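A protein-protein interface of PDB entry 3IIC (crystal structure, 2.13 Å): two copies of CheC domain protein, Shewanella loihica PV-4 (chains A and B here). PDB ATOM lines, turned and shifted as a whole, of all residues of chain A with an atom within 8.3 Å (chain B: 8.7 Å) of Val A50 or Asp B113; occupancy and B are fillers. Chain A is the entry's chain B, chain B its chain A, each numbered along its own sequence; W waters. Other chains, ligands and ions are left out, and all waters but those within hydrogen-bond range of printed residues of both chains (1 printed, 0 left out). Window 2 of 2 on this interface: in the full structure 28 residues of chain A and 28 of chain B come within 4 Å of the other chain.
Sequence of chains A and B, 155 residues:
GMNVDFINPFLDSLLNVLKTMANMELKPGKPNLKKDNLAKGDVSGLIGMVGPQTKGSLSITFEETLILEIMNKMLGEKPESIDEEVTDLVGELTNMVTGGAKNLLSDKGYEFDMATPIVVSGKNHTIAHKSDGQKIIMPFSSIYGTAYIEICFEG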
ATOM      1  N   ILE A  47      30.076   6.905 -12.364  1.00  0.00           N
ATOM      2  CA  ILE A  47      29.069   7.640 -11.606  1.00  0.00           C
ATOM      3  C   ILE A  47      28.202   8.485 -12.548  1.00  0.00           C
ATOM      4  O   ILE A  47      28.706   9.124 -13.502  1.00  0.00           O
ATOM      5  CB  ILE A  47      29.750   8.497 -10.487  1.00  0.00           C
ATOM      6  CG1 ILE A  47      28.726   8.955  -9.435  1.00  0.00           C
ATOM      7  CG2 ILE A  47      30.579   9.626 -11.090  1.00  0.00           C
ATOM      8  CD1 ILE A  47      29.336   9.674  -8.232  1.00  0.00           C
ATOM      9  N   GLY A  48      26.898   8.440 -12.295  1.00  0.00           N
ATOM     10  CA  GLY A  48      25.904   9.191 -13.037  1.00  0.00           C
ATOM     11  C   GLY A  48      25.629  10.534 -12.384  1.00  0.00           C
ATOM     12  O   GLY A  48      25.674  10.659 -11.144  1.00  0.00           O
ATOM     13  N   MET A  49      25.318  11.526 -13.214  1.00  0.00           N
ATOM     14  CA  MET A  49      25.020  12.887 -12.765  1.00  0.00           C
ATOM     15  C   MET A  49      23.731  13.393 -13.407  1.00  0.00           C
ATOM     16  O   MET A  49      23.502  13.163 -14.589  1.00  0.00           O
ATOM     17  CB  MET A  49      26.169  13.823 -13.126  1.00  0.00           C
ATOM     18  CG  MET A  49      27.520  13.468 -12.450  1.00  0.00           C
ATOM     19  SD  MET A  49      28.956  14.589 -13.066  1.00  0.00           S
ATOM     20  CE  MET A  49      29.416  13.639 -14.713  1.00  0.00           C
ATOM     21  N   VAL A  50      22.899  14.061 -12.605  1.00  0.00           N
ATOM     22  CA  VAL A  50      21.645  14.670 -13.048  1.00  0.00           C
ATOM     23  C   VAL A  50      21.580  16.114 -12.525  1.00  0.00           C
ATOM     24  O   VAL A  50      21.869  16.356 -11.358  1.00  0.00           O
ATOM     25  CB  VAL A  50      20.411  13.884 -12.529  1.00  0.00           C
ATOM     26  CG1 VAL A  50      19.120  14.454 -13.108  1.00  0.00           C
ATOM     27  CG2 VAL A  50      20.534  12.412 -12.878  1.00  0.00           C
ATOM     28  N   GLY A  51      21.271  17.057 -13.410  1.00  0.00           N
ATOM     29  CA  GLY A  51      21.048  18.474 -13.054  1.00  0.00           C
ATOM     30  C   GLY A  51      19.718  18.935 -13.644  1.00  0.00           C
ATOM     31  O   GLY A  51      19.034  18.137 -14.296  1.00  0.00           O
ATOM     32  N   PRO A  52      19.321  20.210 -13.405  1.00  0.00           N
ATOM     33  CA  PRO A  52      18.064  20.732 -13.982  1.00  0.00           C
ATOM     34  C   PRO A  52      18.105  20.730 -15.524  1.00  0.00           C
ATOM     35  O   PRO A  52      18.924  21.441 -16.125  1.00  0.00           O
ATOM     36  CB  PRO A  52      17.957  22.156 -13.413  1.00  0.00           C
ATOM     37  CG  PRO A  52      19.247  22.464 -12.812  1.00  0.00           C
ATOM     38  CD  PRO A  52      19.976  21.192 -12.524  1.00  0.00           C
ATOM     39  N   GLN A  53      17.230  19.919 -16.128  1.00  0.00           N
ATOM     40  CA  GLN A  53      17.190  19.653 -17.589  1.00  0.00           C
ATOM     41  C   GLN A  53      18.541  19.124 -18.181  1.00  0.00           C
ATOM     42  O   GLN A  53      18.807  19.285 -19.377  1.00  0.00           O
ATOM     43  CB  GLN A  53      16.631  20.857 -18.379  1.00  0.00           C
ATOM     44  CG  GLN A  53      15.093  21.008 -18.369  1.00  0.00           C
ATOM     45  CD  GLN A  53      14.509  21.640 -17.105  1.00  0.00           C
ATOM     46  OE1 GLN A  53      15.080  21.559 -16.014  1.00  0.00           O
ATOM     47  NE2 GLN A  53      13.346  22.267 -17.254  1.00  0.00           N
ATOM     48  N   THR A  54      19.372  18.482 -17.349  1.00  0.00           N
ATOM     49  CA  THR A  54      20.686  17.970 -17.768  1.00  0.00           C
ATOM     50  C   THR A  54      20.974  16.598 -17.144  1.00  0.00           C
ATOM     51  O   THR A  54      20.559  16.312 -16.014  1.00  0.00           O
ATOM     52  CB  THR A  54      21.865  18.937 -17.380  1.00  0.00           C
ATOM     53  OG1 THR A  54      22.168  18.831 -15.980  1.00  0.00           O
ATOM     54  CG2 THR A  54      21.561  20.409 -17.745  1.00  0.00           C
ATOM     55  N   LYS A  55      21.665  15.747 -17.894  1.00  0.00           N
ATOM     56  CA  LYS A  55      22.090  14.457 -17.379  1.00  0.00           C
ATOM     57  C   LYS A  55      23.424  14.056 -17.972  1.00  0.00           C
ATOM     58  O   LYS A  55      23.722  14.378 -19.121  1.00  0.00           O
ATOM     59  CB  LYS A  55      21.007  13.385 -17.527  1.00  0.00           C
ATOM     60  CG  LYS A  55      20.432  13.142 -18.907  1.00  0.00           C
ATOM     61  CD  LYS A  55      19.395  12.022 -18.805  1.00  0.00           C
ATOM     62  CE  LYS A  55      18.857  11.584 -20.132  1.00  0.00           C
ATOM     63  NZ  LYS A  55      17.991  10.370 -19.981  1.00  0.00           N
ATOM     64  N   GLY A  56      24.230  13.366 -17.168  1.00  0.00           N
ATOM     65  CA  GLY A  56      25.563  12.960 -17.582  1.00  0.00           C
ATOM     66  C   GLY A  56      26.163  11.789 -16.855  1.00  0.00           C
ATOM     67  O   GLY A  56      25.489  11.118 -16.088  1.00  0.00           O
ATOM     68  N   SER A  57      27.443  11.547 -17.130  1.00  0.00           N
ATOM     69  CA  SER A  57      28.174  10.408 -16.582  1.00  0.00           C
ATOM     70  C   SER A  57      29.669  10.633 -16.627  1.00  0.00           C
ATOM     71  O   SER A  57      30.174  11.291 -17.534  1.00  0.00           O
ATOM     72  CB  SER A  57      27.823   9.129 -17.343  1.00  0.00           C
ATOM     73  OG  SER A  57      27.981   9.321 -18.732  1.00  0.00           O
ATOM     74  N   LYS A 102      31.964  18.938  -8.351  1.00  0.00           N
ATOM     75  CA  LYS A 102      30.631  19.478  -8.015  1.00  0.00           C
ATOM     76  C   LYS A 102      30.715  20.822  -7.260  1.00  0.00           C
ATOM     77  O   LYS A 102      29.940  21.733  -7.563  1.00  0.00           O
ATOM     78  CB  LYS A 102      29.760  18.461  -7.233  1.00  0.00           C
ATOM     79  CG  LYS A 102      28.372  19.016  -6.823  1.00  0.00           C
ATOM     80  CD  LYS A 102      27.432  18.051  -6.084  1.00  0.00           C
ATOM     81  CE  LYS A 102      26.266  18.894  -5.484  1.00  0.00           C
ATOM     82  NZ  LYS A 102      25.076  18.138  -5.017  1.00  0.00           N
ATOM     83  N   GLU A 111      24.960  23.231 -11.607  1.00  0.00           N
ATOM     84  CA  GLU A 111      24.462  22.439 -10.479  1.00  0.00           C
ATOM     85  C   GLU A 111      24.071  21.041 -10.933  1.00  0.00           C
ATOM     86  O   GLU A 111      23.448  20.872 -11.993  1.00  0.00           O
ATOM     87  CB  GLU A 111      23.239  23.108  -9.867  1.00  0.00           C
ATOM     88  CG  GLU A 111      23.452  24.557  -9.555  1.00  0.00           C
ATOM     89  CD  GLU A 111      24.670  24.786  -8.692  1.00  0.00           C
ATOM     90  OE1 GLU A 111      25.054  23.865  -7.940  1.00  0.00           O
ATOM     91  OE2 GLU A 111      25.231  25.903  -8.752  1.00  0.00           O
ATOM     92  N   PHE A 112      24.447  20.037 -10.144  1.00  0.00           N
ATOM     93  CA  PHE A 112      24.092  18.640 -10.417  1.00  0.00           C
ATOM     94  C   PHE A 112      24.207  17.806  -9.148  1.00  0.00           C
ATOM     95  O   PHE A 112      24.945  18.167  -8.233  1.00  0.00           O
ATOM     96  CB  PHE A 112      24.939  18.026 -11.546  1.00  0.00           C
ATOM     97  CG  PHE A 112      26.405  17.842 -11.211  1.00  0.00           C
ATOM     98  CD1 PHE A 112      26.857  16.667 -10.583  1.00  0.00           C
ATOM     99  CD2 PHE A 112      27.345  18.820 -11.560  1.00  0.00           C
ATOM    100  CE1 PHE A 112      28.205  16.480 -10.280  1.00  0.00           C
ATOM    101  CE2 PHE A 112      28.719  18.639 -11.271  1.00  0.00           C
ATOM    102  CZ  PHE A 112      29.145  17.472 -10.638  1.00  0.00           C
ATOM    103  N   ASP A 113      23.447  16.716  -9.116  1.00  0.00           N
ATOM    104  CA  ASP A 113      23.475  15.727  -8.055  1.00  0.00           C
ATOM    105  C   ASP A 113      24.096  14.468  -8.648  1.00  0.00           C
ATOM    106  O   ASP A 113      23.884  14.130  -9.818  1.00  0.00           O
ATOM    107  CB  ASP A 113      22.065  15.436  -7.543  1.00  0.00           C
ATOM    108  CG  ASP A 113      21.497  16.573  -6.728  1.00  0.00           C
ATOM    109  OD1 ASP A 113      22.255  17.139  -5.890  1.00  0.00           O
ATOM    110  OD2 ASP A 113      20.285  16.870  -6.907  1.00  0.00           O
ATOM    111  N   MET A 114      24.872  13.775  -7.834  1.00  0.00           N
ATOM    112  CA  MET A 114      25.562  12.594  -8.281  1.00  0.00           C
ATOM    113  C   MET A 114      24.853  11.387  -7.700  1.00  0.00           C
ATOM    114  O   MET A 114      24.284  11.456  -6.616  1.00  0.00           O
ATOM    115  CB  MET A 114      27.055  12.667  -7.936  1.00  0.00           C
ATOM    116  CG  MET A 114      27.424  12.651  -6.466  1.00  0.00           C
ATOM    117  SD  MET A 114      29.215  13.401  -6.230  1.00  0.00           S
ATOM    118  CE  MET A 114      28.836  15.179  -6.637  1.00  0.00           C
ATOM    119  N   ALA A 115      24.869  10.301  -8.458  1.00  0.00           N
ATOM    120  CA  ALA A 115      24.301   9.037  -8.050  1.00  0.00           C
ATOM    121  C   ALA A 115      25.355   8.274  -7.251  1.00  0.00           C
ATOM    122  O   ALA A 115      26.355   8.846  -6.848  1.00  0.00           O
ATOM    123  CB  ALA A 115      23.850   8.267  -9.258  1.00  0.00           C
ATOM    124  N   PHE A 153      27.902  14.567 -21.143  1.00  0.00           N
ATOM    125  CA  PHE A 153      26.726  15.371 -20.733  1.00  0.00           C
ATOM    126  C   PHE A 153      25.777  15.743 -21.832  1.00  0.00           C
ATOM    127  O   PHE A 153      26.209  16.035 -22.934  1.00  0.00           O
ATOM    128  CB  PHE A 153      27.123  16.669 -20.002  1.00  0.00           C
ATOM    129  CG  PHE A 153      26.913  16.605 -18.528  1.00  0.00           C
ATOM    130  CD1 PHE A 153      25.617  16.763 -18.010  1.00  0.00           C
ATOM    131  CD2 PHE A 153      27.965  16.358 -17.654  1.00  0.00           C
ATOM    132  CE1 PHE A 153      25.364  16.694 -16.628  1.00  0.00           C
ATOM    133  CE2 PHE A 153      27.734  16.276 -16.259  1.00  0.00           C
ATOM    134  CZ  PHE A 153      26.418  16.450 -15.746  1.00  0.00           C
ATOM    135  N   GLU A 154      24.487  15.744 -21.482  1.00  0.00           N
ATOM    136  CA  GLU A 154      23.376  16.181 -22.336  1.00  0.00           C
ATOM    137  C   GLU A 154      22.779  17.437 -21.706  1.00  0.00           C
ATOM    138  O   GLU A 154      22.763  17.560 -20.469  1.00  0.00           O
ATOM    139  CB  GLU A 154      22.274  15.118 -22.404  1.00  0.00           C
ATOM    140  CG  GLU A 154      22.735  13.771 -22.914  1.00  0.00           C
ATOM    141  CD  GLU A 154      21.616  12.736 -23.057  1.00  0.00           C
ATOM    142  OE1 GLU A 154      20.451  13.002 -22.691  1.00  0.00           O
ATOM    143  OE2 GLU A 154      21.917  11.629 -23.537  1.00  0.00           O
ATOM    144  N   ILE B  47      23.606   2.524 -15.004  1.00  0.00           N
ATOM    145  CA  ILE B  47      22.931   3.807 -14.973  1.00  0.00           C
ATOM    146  C   ILE B  47      22.656   4.265 -13.518  1.00  0.00           C
ATOM    147  O   ILE B  47      22.214   3.458 -12.643  1.00  0.00           O
ATOM    148  CB  ILE B  47      21.610   3.728 -15.793  1.00  0.00           C
ATOM    149  CG1 ILE B  47      21.115   5.125 -16.177  1.00  0.00           C
ATOM    150  CG2 ILE B  47      20.477   2.910 -15.014  1.00  0.00           C
ATOM    151  CD1 ILE B  47      19.887   5.095 -17.152  1.00  0.00           C
ATOM    152  N   GLY B  48      22.954   5.541 -13.280  1.00  0.00           N
ATOM    153  CA  GLY B  48      22.744   6.163 -12.003  1.00  0.00           C
ATOM    154  C   GLY B  48      21.358   6.795 -11.914  1.00  0.00           C
ATOM    155  O   GLY B  48      20.746   7.164 -12.933  1.00  0.00           O
ATOM    156  N   MET B  49      20.894   6.919 -10.675  1.00  0.00           N
ATOM    157  CA  MET B  49      19.587   7.472 -10.325  1.00  0.00           C
ATOM    158  C   MET B  49      19.731   8.413  -9.137  1.00  0.00           C
ATOM    159  O   MET B  49      20.511   8.132  -8.213  1.00  0.00           O
ATOM    160  CB  MET B  49      18.604   6.347  -9.975  1.00  0.00           C
ATOM    161  CG  MET B  49      18.081   5.643 -11.172  1.00  0.00           C
ATOM    162  SD  MET B  49      17.135   4.012 -10.826  1.00  0.00           S
ATOM    163  CE  MET B  49      18.350   2.925  -9.802  1.00  0.00           C
ATOM    164  N   VAL B  50      18.992   9.523  -9.195  1.00  0.00           N
ATOM    165  CA  VAL B  50      18.965  10.561  -8.164  1.00  0.00           C
ATOM    166  C   VAL B  50      17.518  11.012  -7.985  1.00  0.00           C
ATOM    167  O   VAL B  50      16.874  11.409  -8.958  1.00  0.00           O
ATOM    168  CB  VAL B  50      19.804  11.822  -8.595  1.00  0.00           C
ATOM    169  CG1 VAL B  50      19.698  12.982  -7.562  1.00  0.00           C
ATOM    170  CG2 VAL B  50      21.277  11.452  -8.873  1.00  0.00           C
ATOM    171  N   GLY B  51      17.012  10.941  -6.756  1.00  0.00           N
ATOM    172  CA  GLY B  51      15.686  11.486  -6.415  1.00  0.00           C
ATOM    173  C   GLY B  51      15.876  12.521  -5.326  1.00  0.00           C
ATOM    174  O   GLY B  51      17.012  12.775  -4.923  1.00  0.00           O
ATOM    175  N   PRO B  52      14.780  13.150  -4.857  1.00  0.00           N
ATOM    176  CA  PRO B  52      14.915  14.120  -3.749  1.00  0.00           C
ATOM    177  C   PRO B  52      15.415  13.442  -2.451  1.00  0.00           C
ATOM    178  O   PRO B  52      14.763  12.536  -1.929  1.00  0.00           O
ATOM    179  CB  PRO B  52      13.508  14.702  -3.621  1.00  0.00           C
ATOM    180  CG  PRO B  52      12.919  14.564  -4.980  1.00  0.00           C
ATOM    181  CD  PRO B  52      13.459  13.272  -5.516  1.00  0.00           C
ATOM    182  N   THR B  54      17.736  11.228  -2.171  1.00  0.00           N
ATOM    183  CA  THR B  54      18.027   9.799  -2.409  1.00  0.00           C
ATOM    184  C   THR B  54      18.927   9.624  -3.650  1.00  0.00           C
ATOM    185  O   THR B  54      18.909  10.449  -4.590  1.00  0.00           O
ATOM    186  CB  THR B  54      16.740   8.926  -2.624  1.00  0.00           C
ATOM    187  OG1 THR B  54      16.143   9.239  -3.891  1.00  0.00           O
ATOM    188  CG2 THR B  54      15.705   9.128  -1.510  1.00  0.00           C
ATOM    189  N   LYS B  55      19.719   8.562  -3.631  1.00  0.00           N
ATOM    190  CA  LYS B  55      20.563   8.221  -4.757  1.00  0.00           C
ATOM    191  C   LYS B  55      20.689   6.694  -4.918  1.00  0.00           C
ATOM    192  O   LYS B  55      20.598   5.932  -3.938  1.00  0.00           O
ATOM    193  CB  LYS B  55      21.907   8.961  -4.698  1.00  0.00           C
ATOM    194  CG  LYS B  55      22.735   8.748  -3.462  1.00  0.00           C
ATOM    195  CD  LYS B  55      24.069   9.491  -3.512  1.00  0.00           C
ATOM    196  CE  LYS B  55      23.907  10.994  -3.355  1.00  0.00           C
ATOM    197  NZ  LYS B  55      25.226  11.681  -3.216  1.00  0.00           N
ATOM    198  N   GLY B  56      20.843   6.266  -6.167  1.00  0.00           N
ATOM    199  CA  GLY B  56      20.915   4.857  -6.498  1.00  0.00           C
ATOM    200  C   GLY B  56      21.587   4.536  -7.801  1.00  0.00           C
ATOM    201  O   GLY B  56      22.092   5.426  -8.510  1.00  0.00           O
ATOM    202  N   SER B  57      21.570   3.250  -8.111  1.00  0.00           N
ATOM    203  CA  SER B  57      22.230   2.738  -9.297  1.00  0.00           C
ATOM    204  C   SER B  57      21.676   1.405  -9.753  1.00  0.00           C
ATOM    205  O   SER B  57      21.197   0.607  -8.947  1.00  0.00           O
ATOM    206  CB  SER B  57      23.752   2.641  -9.047  1.00  0.00           C
ATOM    207  OG  SER B  57      24.046   1.929  -7.843  1.00  0.00           O
ATOM    208  N   THR B  98      15.109   1.002 -17.052  1.00  0.00           N
ATOM    209  CA  THR B  98      15.093   2.075 -16.034  1.00  0.00           C
ATOM    210  C   THR B  98      13.892   3.056 -16.205  1.00  0.00           C
ATOM    211  O   THR B  98      13.183   3.350 -15.228  1.00  0.00           O
ATOM    212  CB  THR B  98      16.440   2.861 -16.004  1.00  0.00           C
ATOM    213  OG1 THR B  98      17.516   1.929 -16.097  1.00  0.00           O
ATOM    214  CG2 THR B  98      16.580   3.644 -14.719  1.00  0.00           C
ATOM    215  N   LYS B 102      10.906   3.733 -13.770  1.00  0.00           N
ATOM    216  CA  LYS B 102      10.703   5.159 -13.421  1.00  0.00           C
ATOM    217  C   LYS B 102       9.211   5.511 -13.439  1.00  0.00           C
ATOM    218  O   LYS B 102       8.714   6.122 -12.481  1.00  0.00           O
ATOM    219  CB  LYS B 102      11.462   6.094 -14.404  1.00  0.00           C
ATOM    220  CG  LYS B 102      11.601   7.555 -13.982  1.00  0.00           C
ATOM    221  CD  LYS B 102      11.701   8.483 -15.176  1.00  0.00           C
ATOM    222  CE  LYS B 102      12.072   9.905 -14.815  1.00  0.00           C
ATOM    223  NZ  LYS B 102      11.182  10.482 -13.790  1.00  0.00           N
ATOM    224  N   TYR B 110       7.316   7.087  -5.670  1.00  0.00           N
ATOM    225  CA  TYR B 110       8.788   7.095  -5.738  1.00  0.00           C
ATOM    226  C   TYR B 110       9.179   7.874  -6.994  1.00  0.00           C
ATOM    227  O   TYR B 110       8.785   7.496  -8.079  1.00  0.00           O
ATOM    228  CB  TYR B 110       9.359   5.672  -5.786  1.00  0.00           C
ATOM    229  CG  TYR B 110       9.044   4.789  -4.583  1.00  0.00           C
ATOM    230  CD1 TYR B 110       9.891   4.760  -3.458  1.00  0.00           C
ATOM    231  CD2 TYR B 110       7.896   3.964  -4.564  1.00  0.00           C
ATOM    232  CE1 TYR B 110       9.612   3.928  -2.357  1.00  0.00           C
ATOM    233  CE2 TYR B 110       7.613   3.132  -3.459  1.00  0.00           C
ATOM    234  CZ  TYR B 110       8.480   3.122  -2.373  1.00  0.00           C
ATOM    235  OH  TYR B 110       8.207   2.320  -1.298  1.00  0.00           O
ATOM    236  N   GLU B 111       9.919   8.971  -6.839  1.00  0.00           N
ATOM    237  CA  GLU B 111      10.354   9.809  -7.961  1.00  0.00           C
ATOM    238  C   GLU B 111      11.888   9.848  -8.036  1.00  0.00           C
ATOM    239  O   GLU B 111      12.583   9.934  -7.013  1.00  0.00           O
ATOM    240  CB  GLU B 111       9.830  11.244  -7.819  1.00  0.00           C
ATOM    241  CG  GLU B 111       8.286  11.419  -7.718  1.00  0.00           C
ATOM    242  CD  GLU B 111       7.512  11.084  -8.998  1.00  0.00           C
ATOM    243  OE1 GLU B 111       8.018  11.267 -10.124  1.00  0.00           O
ATOM    244  OE2 GLU B 111       6.350  10.663  -8.882  1.00  0.00           O
ATOM    245  N   PHE B 112      12.406   9.767  -9.258  1.00  0.00           N
ATOM    246  CA  PHE B 112      13.838   9.913  -9.516  1.00  0.00           C
ATOM    247  C   PHE B 112      14.101  10.225 -10.974  1.00  0.00           C
ATOM    248  O   PHE B 112      13.285   9.894 -11.839  1.00  0.00           O
ATOM    249  CB  PHE B 112      14.599   8.654  -9.138  1.00  0.00           C
ATOM    250  CG  PHE B 112      14.208   7.445  -9.933  1.00  0.00           C
ATOM    251  CD1 PHE B 112      14.865   7.132 -11.139  1.00  0.00           C
ATOM    252  CD2 PHE B 112      13.201   6.599  -9.469  1.00  0.00           C
ATOM    253  CE1 PHE B 112      14.513   5.991 -11.888  1.00  0.00           C
ATOM    254  CE2 PHE B 112      12.842   5.458 -10.195  1.00  0.00           C
ATOM    255  CZ  PHE B 112      13.526   5.137 -11.411  1.00  0.00           C
ATOM    256  N   ASP B 113      15.229  10.870 -11.223  1.00  0.00           N
ATOM    257  CA  ASP B 113      15.701  11.118 -12.573  1.00  0.00           C
ATOM    258  C   ASP B 113      16.903  10.215 -12.766  1.00  0.00           C
ATOM    259  O   ASP B 113      17.572   9.838 -11.793  1.00  0.00           O
ATOM    260  CB  ASP B 113      16.059  12.582 -12.771  1.00  0.00           C
ATOM    261  CG  ASP B 113      14.853  13.488 -12.643  1.00  0.00           C
ATOM    262  OD1 ASP B 113      13.773  13.154 -13.196  1.00  0.00           O
ATOM    263  OD2 ASP B 113      14.992  14.534 -11.986  1.00  0.00           O
ATOM    264  N   MET B 114      17.186   9.911 -14.026  1.00  0.00           N
ATOM    265  CA  MET B 114      18.254   9.012 -14.391  1.00  0.00           C
ATOM    266  C   MET B 114      19.398   9.723 -15.120  1.00  0.00           C
ATOM    267  O   MET B 114      19.190  10.715 -15.827  1.00  0.00           O
ATOM    268  CB  MET B 114      17.675   7.844 -15.209  1.00  0.00           C
ATOM    269  CG  MET B 114      17.095   8.180 -16.569  1.00  0.00           C
ATOM    270  SD  MET B 114      16.054   6.649 -17.244  1.00  0.00           S
ATOM    271  CE  MET B 114      14.574   6.874 -16.028  1.00  0.00           C
ATOM    272  N   ALA B 115      20.611   9.196 -14.930  1.00  0.00           N
ATOM    273  CA  ALA B 115      21.825   9.707 -15.601  1.00  0.00           C
ATOM    274  C   ALA B 115      21.900   9.112 -17.016  1.00  0.00           C
ATOM    275  O   ALA B 115      20.961   8.463 -17.451  1.00  0.00           O
ATOM    276  CB  ALA B 115      23.074   9.343 -14.794  1.00  0.00           C
ATOM    277  N   THR B 116      22.992   9.390 -17.746  1.00  0.00           N
ATOM    278  CA  THR B 116      23.234   8.775 -19.065  1.00  0.00           C
ATOM    279  C   THR B 116      23.790   7.362 -18.792  1.00  0.00           C
ATOM    280  O   THR B 116      24.521   7.146 -17.828  1.00  0.00           O
ATOM    281  CB  THR B 116      24.188   9.577 -19.971  1.00  0.00           C
ATOM    282  OG1 THR B 116      25.310  10.002 -19.209  1.00  0.00           O
ATOM    283  CG2 THR B 116      23.527  10.792 -20.551  1.00  0.00           C
ATOM    284  N   PHE B 153      20.005   1.294  -3.839  1.00  0.00           N
ATOM    285  CA  PHE B 153      19.370   2.586  -3.513  1.00  0.00           C
ATOM    286  C   PHE B 153      19.536   2.937  -2.038  1.00  0.00           C
ATOM    287  O   PHE B 153      19.507   2.049  -1.208  1.00  0.00           O
ATOM    288  CB  PHE B 153      17.877   2.523  -3.896  1.00  0.00           C
ATOM    289  CG  PHE B 153      17.418   3.700  -4.725  1.00  0.00           C
ATOM    290  CD1 PHE B 153      16.962   4.884  -4.117  1.00  0.00           C
ATOM    291  CD2 PHE B 153      17.470   3.629  -6.123  1.00  0.00           C
ATOM    292  CE1 PHE B 153      16.560   5.983  -4.899  1.00  0.00           C
ATOM    293  CE2 PHE B 153      17.081   4.731  -6.924  1.00  0.00           C
ATOM    294  CZ  PHE B 153      16.614   5.911  -6.306  1.00  0.00           C
HETATM  295  O   HOH W   1      19.530   8.059 -19.772  1.00  0.00           O
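OG1 of Thr B116 sits close to O of Gly A56, 3.3 Å away.
The side-chain hydroxyl (OG1) of Thr B116 is in hydrogen-bond range of the side-chain hydroxyl (OG) of Ser A57 (2.8 Å).
Of the 19 printed residues of chain A, 10 touch a printed residue of chain B.
Among the printed residues, no Asp or Glu carboxylate lies within 4 Å of a Lys or Arg side-chain nitrogen of the other chain.
No residue of chain B comes within 4 Å of Gly A51.
Pro A52 touches none of the printed residues of chain B.
Gln A53 touches none of the printed residues of chain B.
Printed residues of chain B within 4 Å of Ser A57: Thr B116.
Of the printed residues of chain A, Gly B48 touches Ala A115 (3.6 Å).
Of the printed residues of chain A, Asp B113 touches Val A50.
O of Gly B48 is in hydrogen-bond range of N of Ala B115 (2.9 Å).
The backbone NH of Gly B56 is in hydrogen-bond range of the backbone carbonyl oxygen of Met B49 (2.8 Å).
NZ of Lys B102 is in salt-bridge range of OD1 of Asp B113, at 3.8 Å.
The backbone carbonyl oxygen (O) of Gly A48 lies within hydrogen-bond range of the backbone NH (N) of Ala A115.
The backbone NH of Gly A56 sits at hydrogen-bond distance from the backbone carbonyl oxygen of Met A49, at 2.7 Å.
O of Lys A55 is in hydrogen-bond range of N of Glu A154, 2.8 Å away.
Water W1 lies within hydrogen-bond range of O of Ala B115 and NZ of Lys A55.
Gly A48 touches Ala B115.
N of Met A49 touches CB of Ala B115, 3.5 Å away.
Val A50 touches Met B114.
Val A50 touches Ala B115 (CG2 to N, 3.8 Å).
Lys A55 touches Thr B116.
Asp A113 touches Val B50 (CB to CG1, 3.4 Å).
Val B50 touches Met A114.
Lys B55 touches Met A114.
CB of Ala A115 touches O of Gly B56 (3.4 Å).
Glu A154 touches Thr B116.
Gly A48 touches Ala B115, and with the chains exchanged Ala A115 touches Gly B48.
Val A50 touches Ala B115, and with the chains exchanged Ala A115 touches Val B50.
Lys A55 touches Met B114, and with the chains exchanged Met A114 touches Lys B55.
Gly A56 touches Ala B115, and with the chains exchanged Ala A115 touches Gly B56.
17 positions are printed for both chains.
Of the 18 pairs that touch across the chains among the printed residues, 14 have their exchanged pair printed and touching as well.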
